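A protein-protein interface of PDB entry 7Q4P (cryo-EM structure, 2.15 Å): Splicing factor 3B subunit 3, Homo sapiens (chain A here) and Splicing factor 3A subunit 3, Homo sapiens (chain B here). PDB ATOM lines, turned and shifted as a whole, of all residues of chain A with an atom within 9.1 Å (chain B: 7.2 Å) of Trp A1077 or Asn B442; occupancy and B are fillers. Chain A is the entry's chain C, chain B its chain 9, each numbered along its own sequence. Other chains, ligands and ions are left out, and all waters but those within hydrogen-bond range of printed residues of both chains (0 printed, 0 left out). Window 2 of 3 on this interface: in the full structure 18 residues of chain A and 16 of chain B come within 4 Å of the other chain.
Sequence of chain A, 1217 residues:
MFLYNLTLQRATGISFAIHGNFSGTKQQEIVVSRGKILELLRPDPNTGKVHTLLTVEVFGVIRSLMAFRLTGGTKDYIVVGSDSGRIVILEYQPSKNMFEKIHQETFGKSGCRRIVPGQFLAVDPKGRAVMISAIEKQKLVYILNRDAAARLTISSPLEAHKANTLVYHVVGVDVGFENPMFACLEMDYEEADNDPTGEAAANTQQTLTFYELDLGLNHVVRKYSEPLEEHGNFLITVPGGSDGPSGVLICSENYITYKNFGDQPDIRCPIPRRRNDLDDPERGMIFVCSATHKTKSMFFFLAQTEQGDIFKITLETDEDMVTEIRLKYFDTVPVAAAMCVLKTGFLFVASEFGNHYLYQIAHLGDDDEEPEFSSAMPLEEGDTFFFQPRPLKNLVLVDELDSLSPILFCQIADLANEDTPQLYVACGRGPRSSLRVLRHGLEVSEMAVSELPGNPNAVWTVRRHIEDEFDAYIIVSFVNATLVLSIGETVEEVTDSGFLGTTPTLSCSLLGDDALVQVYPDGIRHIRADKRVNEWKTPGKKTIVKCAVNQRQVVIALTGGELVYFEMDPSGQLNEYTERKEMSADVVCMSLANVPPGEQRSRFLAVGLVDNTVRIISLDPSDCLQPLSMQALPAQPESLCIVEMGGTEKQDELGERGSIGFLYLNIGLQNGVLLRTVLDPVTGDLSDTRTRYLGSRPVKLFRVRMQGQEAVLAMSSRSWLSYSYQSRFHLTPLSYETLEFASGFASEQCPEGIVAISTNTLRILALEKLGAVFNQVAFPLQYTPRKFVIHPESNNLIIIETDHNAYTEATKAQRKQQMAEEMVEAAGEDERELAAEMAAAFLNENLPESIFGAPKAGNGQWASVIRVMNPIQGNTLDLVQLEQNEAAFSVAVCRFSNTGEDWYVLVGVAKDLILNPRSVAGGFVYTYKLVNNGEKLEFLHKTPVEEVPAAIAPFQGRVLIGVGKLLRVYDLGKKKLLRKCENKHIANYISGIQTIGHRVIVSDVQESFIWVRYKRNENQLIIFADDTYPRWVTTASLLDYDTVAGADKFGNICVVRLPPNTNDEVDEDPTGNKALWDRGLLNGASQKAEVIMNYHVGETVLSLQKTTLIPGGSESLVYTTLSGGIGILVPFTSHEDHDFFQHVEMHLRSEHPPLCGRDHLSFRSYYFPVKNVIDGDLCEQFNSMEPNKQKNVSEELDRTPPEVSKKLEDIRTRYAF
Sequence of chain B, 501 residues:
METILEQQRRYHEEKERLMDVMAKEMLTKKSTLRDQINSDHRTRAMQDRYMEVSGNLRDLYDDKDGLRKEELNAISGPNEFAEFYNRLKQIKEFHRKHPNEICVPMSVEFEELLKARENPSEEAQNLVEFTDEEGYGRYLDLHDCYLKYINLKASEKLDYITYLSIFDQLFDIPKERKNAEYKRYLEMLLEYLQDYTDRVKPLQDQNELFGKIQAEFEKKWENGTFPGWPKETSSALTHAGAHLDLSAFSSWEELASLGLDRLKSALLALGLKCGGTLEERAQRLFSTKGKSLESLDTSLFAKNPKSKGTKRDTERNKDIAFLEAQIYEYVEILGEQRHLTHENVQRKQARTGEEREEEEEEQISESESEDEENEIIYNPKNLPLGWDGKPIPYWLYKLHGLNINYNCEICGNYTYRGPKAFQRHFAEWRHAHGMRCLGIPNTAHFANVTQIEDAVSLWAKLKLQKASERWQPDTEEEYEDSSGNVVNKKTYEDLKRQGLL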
ATOM      1  N   ASP A1069      25.311  17.930  -6.370  1.00  0.00           N
ATOM      2  CA  ASP A1069      25.461  17.043  -5.227  1.00  0.00           C
ATOM      3  C   ASP A1069      26.840  16.386  -5.287  1.00  0.00           C
ATOM      4  O   ASP A1069      27.174  15.750  -6.286  1.00  0.00           O
ATOM      5  CB  ASP A1069      24.317  16.027  -5.157  1.00  0.00           C
ATOM      6  CG  ASP A1069      24.271  15.232  -3.863  1.00  0.00           C
ATOM      7  OD1 ASP A1069      24.180  15.859  -2.786  1.00  0.00           O
ATOM      8  OD2 ASP A1069      24.324  13.988  -3.940  1.00  0.00           O
ATOM      9  N   THR A1071      28.111  13.846  -3.587  1.00  0.00           N
ATOM     10  CA  THR A1071      27.996  12.398  -3.505  1.00  0.00           C
ATOM     11  C   THR A1071      27.386  11.856  -4.796  1.00  0.00           C
ATOM     12  O   THR A1071      27.790  10.797  -5.275  1.00  0.00           O
ATOM     13  CB  THR A1071      27.207  11.958  -2.264  1.00  0.00           C
ATOM     14  OG1 THR A1071      25.958  12.651  -2.239  1.00  0.00           O
ATOM     15  CG2 THR A1071      27.952  12.192  -0.966  1.00  0.00           C
ATOM     16  N   GLY A1072      26.413  12.597  -5.343  1.00  0.00           N
ATOM     17  CA  GLY A1072      25.721  12.229  -6.569  1.00  0.00           C
ATOM     18  C   GLY A1072      24.566  11.266  -6.307  1.00  0.00           C
ATOM     19  O   GLY A1072      24.406  10.280  -7.024  1.00  0.00           O
ATOM     20  N   ASN A1073      23.775  11.574  -5.271  1.00  0.00           N
ATOM     21  CA  ASN A1073      22.616  10.783  -4.884  1.00  0.00           C
ATOM     22  C   ASN A1073      21.336  11.543  -5.223  1.00  0.00           C
ATOM     23  O   ASN A1073      20.319  10.926  -5.536  1.00  0.00           O
ATOM     24  CB  ASN A1073      22.655  10.396  -3.402  1.00  0.00           C
ATOM     25  CG  ASN A1073      23.755   9.412  -3.061  1.00  0.00           C
ATOM     26  OD1 ASN A1073      23.909   8.382  -3.717  1.00  0.00           O
ATOM     27  ND2 ASN A1073      24.515   9.708  -2.019  1.00  0.00           N
ATOM     28  N   LYS A1074      21.411  12.881  -5.164  1.00  0.00           N
ATOM     29  CA  LYS A1074      20.280  13.771  -5.384  1.00  0.00           C
ATOM     30  C   LYS A1074      19.887  13.792  -6.862  1.00  0.00           C
ATOM     31  O   LYS A1074      18.751  14.132  -7.189  1.00  0.00           O
ATOM     32  CB  LYS A1074      20.601  15.182  -4.880  1.00  0.00           C
ATOM     33  CG  LYS A1074      20.564  15.361  -3.368  1.00  0.00           C
ATOM     34  CD  LYS A1074      20.812  16.789  -2.926  1.00  0.00           C
ATOM     35  CE  LYS A1074      20.734  16.969  -1.425  1.00  0.00           C
ATOM     36  NZ  LYS A1074      20.988  18.374  -1.026  1.00  0.00           N
ATOM     37  N   ALA A1075      20.835  13.425  -7.736  1.00  0.00           N
ATOM     38  CA  ALA A1075      20.630  13.372  -9.177  1.00  0.00           C
ATOM     39  C   ALA A1075      19.653  12.255  -9.543  1.00  0.00           C
ATOM     40  O   ALA A1075      18.933  12.365 -10.535  1.00  0.00           O
ATOM     41  CB  ALA A1075      21.955  13.200  -9.879  1.00  0.00           C
ATOM     42  N   LEU A1076      19.646  11.185  -8.734  1.00  0.00           N
ATOM     43  CA  LEU A1076      18.775  10.036  -8.929  1.00  0.00           C
ATOM     44  C   LEU A1076      17.352  10.372  -8.489  1.00  0.00           C
ATOM     45  O   LEU A1076      16.394   9.901  -9.100  1.00  0.00           O
ATOM     46  CB  LEU A1076      19.328   8.844  -8.139  1.00  0.00           C
ATOM     47  CG  LEU A1076      20.566   8.162  -8.723  1.00  0.00           C
ATOM     48  CD1 LEU A1076      21.422   7.561  -7.619  1.00  0.00           C
ATOM     49  CD2 LEU A1076      20.183   7.094  -9.740  1.00  0.00           C
ATOM     50  N   TRP A1077      17.232  11.188  -7.431  1.00  0.00           N
ATOM     51  CA  TRP A1077      15.950  11.526  -6.831  1.00  0.00           C
ATOM     52  C   TRP A1077      15.279  12.676  -7.583  1.00  0.00           C
ATOM     53  O   TRP A1077      14.109  12.570  -7.946  1.00  0.00           O
ATOM     54  CB  TRP A1077      16.102  11.826  -5.333  1.00  0.00           C
ATOM     55  CG  TRP A1077      16.447  10.626  -4.506  1.00  0.00           C
ATOM     56  CD1 TRP A1077      17.655  10.335  -3.941  1.00  0.00           C
ATOM     57  CD2 TRP A1077      15.569   9.542  -4.148  1.00  0.00           C
ATOM     58  NE1 TRP A1077      17.592   9.150  -3.259  1.00  0.00           N
ATOM     59  CE2 TRP A1077      16.326   8.639  -3.367  1.00  0.00           C
ATOM     60  CE3 TRP A1077      14.224   9.243  -4.409  1.00  0.00           C
ATOM     61  CZ2 TRP A1077      15.781   7.462  -2.848  1.00  0.00           C
ATOM     62  CZ3 TRP A1077      13.686   8.079  -3.897  1.00  0.00           C
ATOM     63  CH2 TRP A1077      14.456   7.204  -3.126  1.00  0.00           C
ATOM     64  N   ASP A1078      16.030  13.765  -7.800  1.00  0.00           N
ATOM     65  CA  ASP A1078      15.520  14.959  -8.458  1.00  0.00           C
ATOM     66  C   ASP A1078      15.424  14.713  -9.962  1.00  0.00           C
ATOM     67  O   ASP A1078      16.399  14.302 -10.590  1.00  0.00           O
ATOM     68  CB  ASP A1078      16.350  16.200  -8.111  1.00  0.00           C
ATOM     69  CG  ASP A1078      15.758  17.504  -8.623  1.00  0.00           C
ATOM     70  OD1 ASP A1078      14.647  17.864  -8.178  1.00  0.00           O
ATOM     71  OD2 ASP A1078      16.414  18.153  -9.463  1.00  0.00           O
ATOM     72  N   ARG A1079      14.231  14.971 -10.511  1.00  0.00           N
ATOM     73  CA  ARG A1079      13.937  14.779 -11.924  1.00  0.00           C
ATOM     74  C   ARG A1079      13.588  16.118 -12.571  1.00  0.00           C
ATOM     75  O   ARG A1079      13.504  16.215 -13.795  1.00  0.00           O
ATOM     76  CB  ARG A1079      12.837  13.725 -12.095  1.00  0.00           C
ATOM     77  CG  ARG A1079      13.320  12.295 -11.892  1.00  0.00           C
ATOM     78  CD  ARG A1079      12.207  11.292 -11.641  1.00  0.00           C
ATOM     79  NE  ARG A1079      12.747   9.986 -11.279  1.00  0.00           N
ATOM     80  CZ  ARG A1079      13.007   9.572 -10.038  1.00  0.00           C
ATOM     81  NH1 ARG A1079      12.775  10.361  -9.002  1.00  0.00           N
ATOM     82  NH2 ARG A1079      13.504   8.362  -9.841  1.00  0.00           N
ATOM     83  N   GLY A1080      13.400  17.144 -11.731  1.00  0.00           N
ATOM     84  CA  GLY A1080      13.177  18.507 -12.177  1.00  0.00           C
ATOM     85  C   GLY A1080      11.724  18.735 -12.577  1.00  0.00           C
ATOM     86  O   GLY A1080      10.805  18.282 -11.902  1.00  0.00           O
ATOM     87  N   ILE B 410      12.217  -9.286  -4.937  1.00  0.00           N
ATOM     88  CA  ILE B 410      12.910  -8.381  -4.033  1.00  0.00           C
ATOM     89  C   ILE B 410      12.234  -8.480  -2.671  1.00  0.00           C
ATOM     90  O   ILE B 410      12.784  -8.039  -1.667  1.00  0.00           O
ATOM     91  CB  ILE B 410      12.868  -6.938  -4.576  1.00  0.00           C
ATOM     92  CG1 ILE B 410      13.066  -6.869  -6.088  1.00  0.00           C
ATOM     93  CG2 ILE B 410      13.822  -5.999  -3.846  1.00  0.00           C
ATOM     94  CD1 ILE B 410      14.497  -7.017  -6.521  1.00  0.00           C
ATOM     95  N   HIS B 425       3.264  -1.323  -3.653  1.00  0.00           N
ATOM     96  CA  HIS B 425       4.294  -1.866  -2.783  1.00  0.00           C
ATOM     97  C   HIS B 425       5.703  -1.345  -3.079  1.00  0.00           C
ATOM     98  O   HIS B 425       6.541  -1.300  -2.182  1.00  0.00           O
ATOM     99  CB  HIS B 425       4.213  -3.385  -2.760  1.00  0.00           C
ATOM    100  CG  HIS B 425       4.866  -4.079  -3.897  1.00  0.00           C
ATOM    101  ND1 HIS B 425       6.255  -4.193  -4.061  1.00  0.00           N
ATOM    102  CD2 HIS B 425       4.304  -4.775  -4.892  1.00  0.00           C
ATOM    103  CE1 HIS B 425       6.473  -4.883  -5.158  1.00  0.00           C
ATOM    104  NE2 HIS B 425       5.310  -5.253  -5.661  1.00  0.00           N
ATOM    105  N   PHE B 426       5.985  -1.034  -4.350  1.00  0.00           N
ATOM    106  CA  PHE B 426       7.308  -0.569  -4.738  1.00  0.00           C
ATOM    107  C   PHE B 426       7.746   0.666  -3.945  1.00  0.00           C
ATOM    108  O   PHE B 426       8.906   1.072  -4.025  1.00  0.00           O
ATOM    109  CB  PHE B 426       7.372  -0.359  -6.249  1.00  0.00           C
ATOM    110  CG  PHE B 426       7.196  -1.626  -7.032  1.00  0.00           C
ATOM    111  CD1 PHE B 426       8.266  -2.480  -7.206  1.00  0.00           C
ATOM    112  CD2 PHE B 426       5.999  -1.900  -7.666  1.00  0.00           C
ATOM    113  CE1 PHE B 426       8.135  -3.633  -7.955  1.00  0.00           C
ATOM    114  CE2 PHE B 426       5.865  -3.053  -8.423  1.00  0.00           C
ATOM    115  CZ  PHE B 426       6.932  -3.917  -8.561  1.00  0.00           C
ATOM    116  N   ALA B 427       6.822   1.250  -3.179  1.00  0.00           N
ATOM    117  CA  ALA B 427       7.140   2.385  -2.335  1.00  0.00           C
ATOM    118  C   ALA B 427       6.977   2.028  -0.860  1.00  0.00           C
ATOM    119  O   ALA B 427       7.394   2.790   0.012  1.00  0.00           O
ATOM    120  CB  ALA B 427       6.285   3.555  -2.742  1.00  0.00           C
ATOM    121  N   GLU B 428       6.388   0.856  -0.603  1.00  0.00           N
ATOM    122  CA  GLU B 428       6.156   0.343   0.742  1.00  0.00           C
ATOM    123  C   GLU B 428       7.450  -0.220   1.339  1.00  0.00           C
ATOM    124  O   GLU B 428       8.499  -0.185   0.692  1.00  0.00           O
ATOM    125  CB  GLU B 428       5.018  -0.680   0.705  1.00  0.00           C
ATOM    126  CG  GLU B 428       3.642  -0.063   0.487  1.00  0.00           C
ATOM    127  CD  GLU B 428       2.488  -1.050   0.416  1.00  0.00           C
ATOM    128  OE1 GLU B 428       1.750  -1.017  -0.587  1.00  0.00           O
ATOM    129  OE2 GLU B 428       2.321  -1.839   1.371  1.00  0.00           O
ATOM    130  N   TRP B 429       7.357  -0.752   2.570  1.00  0.00           N
ATOM    131  CA  TRP B 429       8.509  -1.108   3.391  1.00  0.00           C
ATOM    132  C   TRP B 429       9.215  -2.371   2.894  1.00  0.00           C
ATOM    133  O   TRP B 429      10.444  -2.426   2.914  1.00  0.00           O
ATOM    134  CB  TRP B 429       8.138  -1.210   4.881  1.00  0.00           C
ATOM    135  CG  TRP B 429       7.426  -2.476   5.269  1.00  0.00           C
ATOM    136  CD1 TRP B 429       7.969  -3.604   5.819  1.00  0.00           C
ATOM    137  CD2 TRP B 429       6.018  -2.742   5.142  1.00  0.00           C
ATOM    138  NE1 TRP B 429       7.006  -4.554   6.028  1.00  0.00           N
ATOM    139  CE2 TRP B 429       5.795  -4.051   5.629  1.00  0.00           C
ATOM    140  CE3 TRP B 429       4.924  -2.005   4.668  1.00  0.00           C
ATOM    141  CZ2 TRP B 429       4.528  -4.632   5.649  1.00  0.00           C
ATOM    142  CZ3 TRP B 429       3.670  -2.580   4.685  1.00  0.00           C
ATOM    143  CH2 TRP B 429       3.477  -3.875   5.174  1.00  0.00           C
ATOM    144  N   HIS B 431       9.502  -3.804   0.020  1.00  0.00           N
ATOM    145  CA  HIS B 431      10.257  -3.674  -1.207  1.00  0.00           C
ATOM    146  C   HIS B 431      11.505  -2.849  -0.932  1.00  0.00           C
ATOM    147  O   HIS B 431      12.560  -3.181  -1.467  1.00  0.00           O
ATOM    148  CB  HIS B 431       9.404  -3.109  -2.347  1.00  0.00           C
ATOM    149  CG  HIS B 431      10.111  -3.203  -3.657  1.00  0.00           C
ATOM    150  ND1 HIS B 431      10.237  -4.383  -4.393  1.00  0.00           N
ATOM    151  CD2 HIS B 431      10.821  -2.268  -4.317  1.00  0.00           C
ATOM    152  CE1 HIS B 431      10.941  -4.131  -5.486  1.00  0.00           C
ATOM    153  NE2 HIS B 431      11.330  -2.844  -5.451  1.00  0.00           N
ATOM    154  N   ALA B 432      11.339  -1.796  -0.114  1.00  0.00           N
ATOM    155  CA  ALA B 432      12.403  -0.894   0.299  1.00  0.00           C
ATOM    156  C   ALA B 432      13.516  -1.653   1.021  1.00  0.00           C
ATOM    157  O   ALA B 432      14.700  -1.411   0.759  1.00  0.00           O
ATOM    158  CB  ALA B 432      11.831   0.194   1.176  1.00  0.00           C
ATOM    159  N   HIS B 433      13.106  -2.561   1.928  1.00  0.00           N
ATOM    160  CA  HIS B 433      14.024  -3.373   2.711  1.00  0.00           C
ATOM    161  C   HIS B 433      14.814  -4.295   1.788  1.00  0.00           C
ATOM    162  O   HIS B 433      15.968  -4.602   2.062  1.00  0.00           O
ATOM    163  CB  HIS B 433      13.292  -4.186   3.794  1.00  0.00           C
ATOM    164  CG  HIS B 433      13.151  -3.469   5.094  1.00  0.00           C
ATOM    165  ND1 HIS B 433      14.140  -3.490   6.059  1.00  0.00           N
ATOM    166  CD2 HIS B 433      12.148  -2.718   5.596  1.00  0.00           C
ATOM    167  CE1 HIS B 433      13.751  -2.782   7.100  1.00  0.00           C
ATOM    168  NE2 HIS B 433      12.532  -2.296   6.841  1.00  0.00           N
ATOM    169  N   MET B 435      15.437  -3.773  -1.329  1.00  0.00           N
ATOM    170  CA  MET B 435      16.301  -2.959  -2.153  1.00  0.00           C
ATOM    171  C   MET B 435      17.502  -2.499  -1.336  1.00  0.00           C
ATOM    172  O   MET B 435      18.571  -2.368  -1.915  1.00  0.00           O
ATOM    173  CB  MET B 435      15.522  -1.761  -2.689  1.00  0.00           C
ATOM    174  CG  MET B 435      14.572  -2.145  -3.805  1.00  0.00           C
ATOM    175  SD  MET B 435      15.356  -2.463  -5.389  1.00  0.00           S
ATOM    176  CE  MET B 435      15.725  -0.770  -5.850  1.00  0.00           C
ATOM    177  N   ARG B 436      17.335  -2.277  -0.017  1.00  0.00           N
ATOM    178  CA  ARG B 436      18.436  -1.934   0.882  1.00  0.00           C
ATOM    179  C   ARG B 436      19.434  -3.089   0.980  1.00  0.00           C
ATOM    180  O   ARG B 436      20.626  -2.839   1.134  1.00  0.00           O
ATOM    181  CB  ARG B 436      17.957  -1.565   2.294  1.00  0.00           C
ATOM    182  CG  ARG B 436      17.339  -0.179   2.419  1.00  0.00           C
ATOM    183  CD  ARG B 436      16.438  -0.072   3.637  1.00  0.00           C
ATOM    184  NE  ARG B 436      15.539   1.075   3.565  1.00  0.00           N
ATOM    185  CZ  ARG B 436      14.503   1.294   4.372  1.00  0.00           C
ATOM    186  NH1 ARG B 436      14.209   0.441   5.340  1.00  0.00           N
ATOM    187  NH2 ARG B 436      13.758   2.372   4.204  1.00  0.00           N
ATOM    188  N   ILE B 440      20.645  -1.031  -3.486  1.00  0.00           N
ATOM    189  CA  ILE B 440      20.081  -0.230  -4.551  1.00  0.00           C
ATOM    190  C   ILE B 440      19.049   0.719  -3.947  1.00  0.00           C
ATOM    191  O   ILE B 440      18.160   0.280  -3.224  1.00  0.00           O
ATOM    192  CB  ILE B 440      19.497  -1.128  -5.662  1.00  0.00           C
ATOM    193  CG1 ILE B 440      20.505  -2.186  -6.111  1.00  0.00           C
ATOM    194  CG2 ILE B 440      19.092  -0.266  -6.843  1.00  0.00           C
ATOM    195  CD1 ILE B 440      19.887  -3.343  -6.838  1.00  0.00           C
ATOM    196  N   PRO B 441      19.149   2.051  -4.179  1.00  0.00           N
ATOM    197  CA  PRO B 441      18.136   3.001  -3.722  1.00  0.00           C
ATOM    198  C   PRO B 441      16.816   2.775  -4.448  1.00  0.00           C
ATOM    199  O   PRO B 441      16.759   2.541  -5.656  1.00  0.00           O
ATOM    200  CB  PRO B 441      18.709   4.388  -4.058  1.00  0.00           C
ATOM    201  CG  PRO B 441      19.666   4.114  -5.191  1.00  0.00           C
ATOM    202  CD  PRO B 441      20.227   2.737  -4.900  1.00  0.00           C
ATOM    203  N   ASN B 442      15.745   2.839  -3.664  1.00  0.00           N
ATOM    204  CA  ASN B 442      14.431   2.481  -4.142  1.00  0.00           C
ATOM    205  C   ASN B 442      13.805   3.699  -4.817  1.00  0.00           C
ATOM    206  O   ASN B 442      13.011   4.424  -4.213  1.00  0.00           O
ATOM    207  CB  ASN B 442      13.673   1.829  -2.992  1.00  0.00           C
ATOM    208  CG  ASN B 442      12.305   1.336  -3.391  1.00  0.00           C
ATOM    209  OD1 ASN B 442      12.152   0.662  -4.409  1.00  0.00           O
ATOM    210  ND2 ASN B 442      11.312   1.691  -2.597  1.00  0.00           N
ATOM    211  N   THR B 443      14.208   3.937  -6.079  1.00  0.00           N
ATOM    212  CA  THR B 443      13.765   5.079  -6.869  1.00  0.00           C
ATOM    213  C   THR B 443      12.647   4.653  -7.820  1.00  0.00           C
ATOM    214  O   THR B 443      12.187   3.518  -7.771  1.00  0.00           O
ATOM    215  CB  THR B 443      14.922   5.751  -7.621  1.00  0.00           C
ATOM    216  OG1 THR B 443      15.601   4.758  -8.381  1.00  0.00           O
ATOM    217  CG2 THR B 443      15.949   6.391  -6.712  1.00  0.00           C
ATOM    218  N   ALA B 444      12.185   5.609  -8.634  1.00  0.00           N
ATOM    219  CA  ALA B 444      11.087   5.379  -9.563  1.00  0.00           C
ATOM    220  C   ALA B 444      11.598   4.588 -10.765  1.00  0.00           C
ATOM    221  O   ALA B 444      10.807   4.049 -11.545  1.00  0.00           O
ATOM    222  CB  ALA B 444      10.472   6.694  -9.978  1.00  0.00           C
ATOM    223  N   HIS B 445      12.932   4.551 -10.884  1.00  0.00           N
ATOM    224  CA  HIS B 445      13.623   3.758 -11.884  1.00  0.00           C
ATOM    225  C   HIS B 445      13.326   2.270 -11.727  1.00  0.00           C
ATOM    226  O   HIS B 445      13.251   1.563 -12.729  1.00  0.00           O
ATOM    227  CB  HIS B 445      15.129   4.001 -11.783  1.00  0.00           C
ATOM    228  CG  HIS B 445      15.526   5.383 -12.166  1.00  0.00           C
ATOM    229  ND1 HIS B 445      15.637   6.409 -11.243  1.00  0.00           N
ATOM    230  CD2 HIS B 445      15.858   5.909 -13.361  1.00  0.00           C
ATOM    231  CE1 HIS B 445      16.012   7.512 -11.857  1.00  0.00           C
ATOM    232  NE2 HIS B 445      16.161   7.229 -13.161  1.00  0.00           N
ATOM    233  N   PHE B 446      13.171   1.806 -10.479  1.00  0.00           N
ATOM    234  CA  PHE B 446      13.112   0.377 -10.214  1.00  0.00           C
ATOM    235  C   PHE B 446      11.713  -0.041  -9.795  1.00  0.00           C
ATOM    236  O   PHE B 446      11.539  -1.102  -9.202  1.00  0.00           O
ATOM    237  CB  PHE B 446      14.053   0.051  -9.059  1.00  0.00           C
ATOM    238  CG  PHE B 446      15.481   0.371  -9.374  1.00  0.00           C
ATOM    239  CD1 PHE B 446      16.276  -0.531 -10.076  1.00  0.00           C
ATOM    240  CD2 PHE B 446      16.023   1.579  -8.962  1.00  0.00           C
ATOM    241  CE1 PHE B 446      17.593  -0.225 -10.379  1.00  0.00           C
ATOM    242  CE2 PHE B 446      17.340   1.881  -9.267  1.00  0.00           C
ATOM    243  CZ  PHE B 446      18.116   0.986  -9.979  1.00  0.00           C
ATOM    244  N   ALA B 447      10.738   0.846 -10.016  1.00  0.00           N
ATOM    245  CA  ALA B 447       9.348   0.442  -9.884  1.00  0.00           C
ATOM    246  C   ALA B 447       9.015  -0.526 -11.012  1.00  0.00           C
ATOM    247  O   ALA B 447       9.466  -0.351 -12.146  1.00  0.00           O
ATOM    248  CB  ALA B 447       8.447   1.642  -9.936  1.00  0.00           C
ATOM    249  N   LYS B 466      24.916   7.918 -14.766  1.00  0.00           N
ATOM    250  CA  LYS B 466      25.010   9.117 -13.948  1.00  0.00           C
ATOM    251  C   LYS B 466      26.467   9.569 -13.799  1.00  0.00           C
ATOM    252  O   LYS B 466      26.725  10.752 -13.611  1.00  0.00           O
ATOM    253  CB  LYS B 466      24.294   8.896 -12.610  1.00  0.00           C
ATOM    254  CG  LYS B 466      22.781   8.676 -12.684  1.00  0.00           C
ATOM    255  CD  LYS B 466      21.947   9.945 -12.771  1.00  0.00           C
ATOM    256  CE  LYS B 466      20.454   9.688 -12.850  1.00  0.00           C
ATOM    257  NZ  LYS B 466      19.681  10.949 -12.954  1.00  0.00           N
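A ring nitrogen (ND1) of His B445 lies within hydrogen-bond range of the guanidinium group of Arg A1079 (3.2 Å). The side-chain amino group (NZ) of Lys B466 sits at hydrogen-bond distance from the backbone carbonyl oxygen (O) of Ala A1075 (2.9 Å). The backbone NH (N) of Ala B444 sits close to the guanidinium group (NH2) of Arg A1079 (3.3 Å).
Hydrophobic or aromatic side chains of chain A within 4 Å of the printed part of chain B: Trp A1077. Of the 20 printed residues of chain B, 5 touch a printed residue of chain A. Hydrophobic or aromatic side chains of chain B that line the printed part of chain A: Ala B444 and His B445. Among the printed residues, no Asp or Glu carboxylate lies within 4 Å of a Lys or Arg side-chain nitrogen of the other chain.
Among the printed residues, merely in contact across the chains: Trp A1077 with Asn B442, Leu A1076 with His B445, Arg A1079 with Thr B443 and Trp A1077 with Thr B443.
Of the printed residues of chain B, Trp A1077 touches Asn B442 and Thr B443. Of the printed residues of chain A, Asn B442 touches Trp A1077 (3.3 Å). No residue of chain A comes within 4 Å of Pro B441. Of chain A, only Trp A1077 (3.97 Å) and Arg A1079 (3.7 Å) come within 4 Å of Thr B443. Of the printed residues of chain B, Arg A1079 touches Thr B443, Ala B444 and His B445. Of the printed residues of chain A, Ala B444 touches Arg A1079 (3.3 Å). Printed residues of chain A within 4 Å of Lys B466: Ala A1075. His B425 touches none of the printed residues of chain A. Lys A1074 touches none of the printed residues of chain B.
O of Phe B426 lies within hydrogen-bond range of ND2 of Asn B442 (2.9 Å). The side-chain hydroxyl (OG1) of Thr B443 is in hydrogen-bond range of a ring nitrogen (ND1) of His B445 (3.3 Å). O of Leu A1076 lies within hydrogen-bond range of NH2 of Arg A1079, 3.4 Å away. O of Trp A1077 is in hydrogen-bond range of NH1 of Arg A1079.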
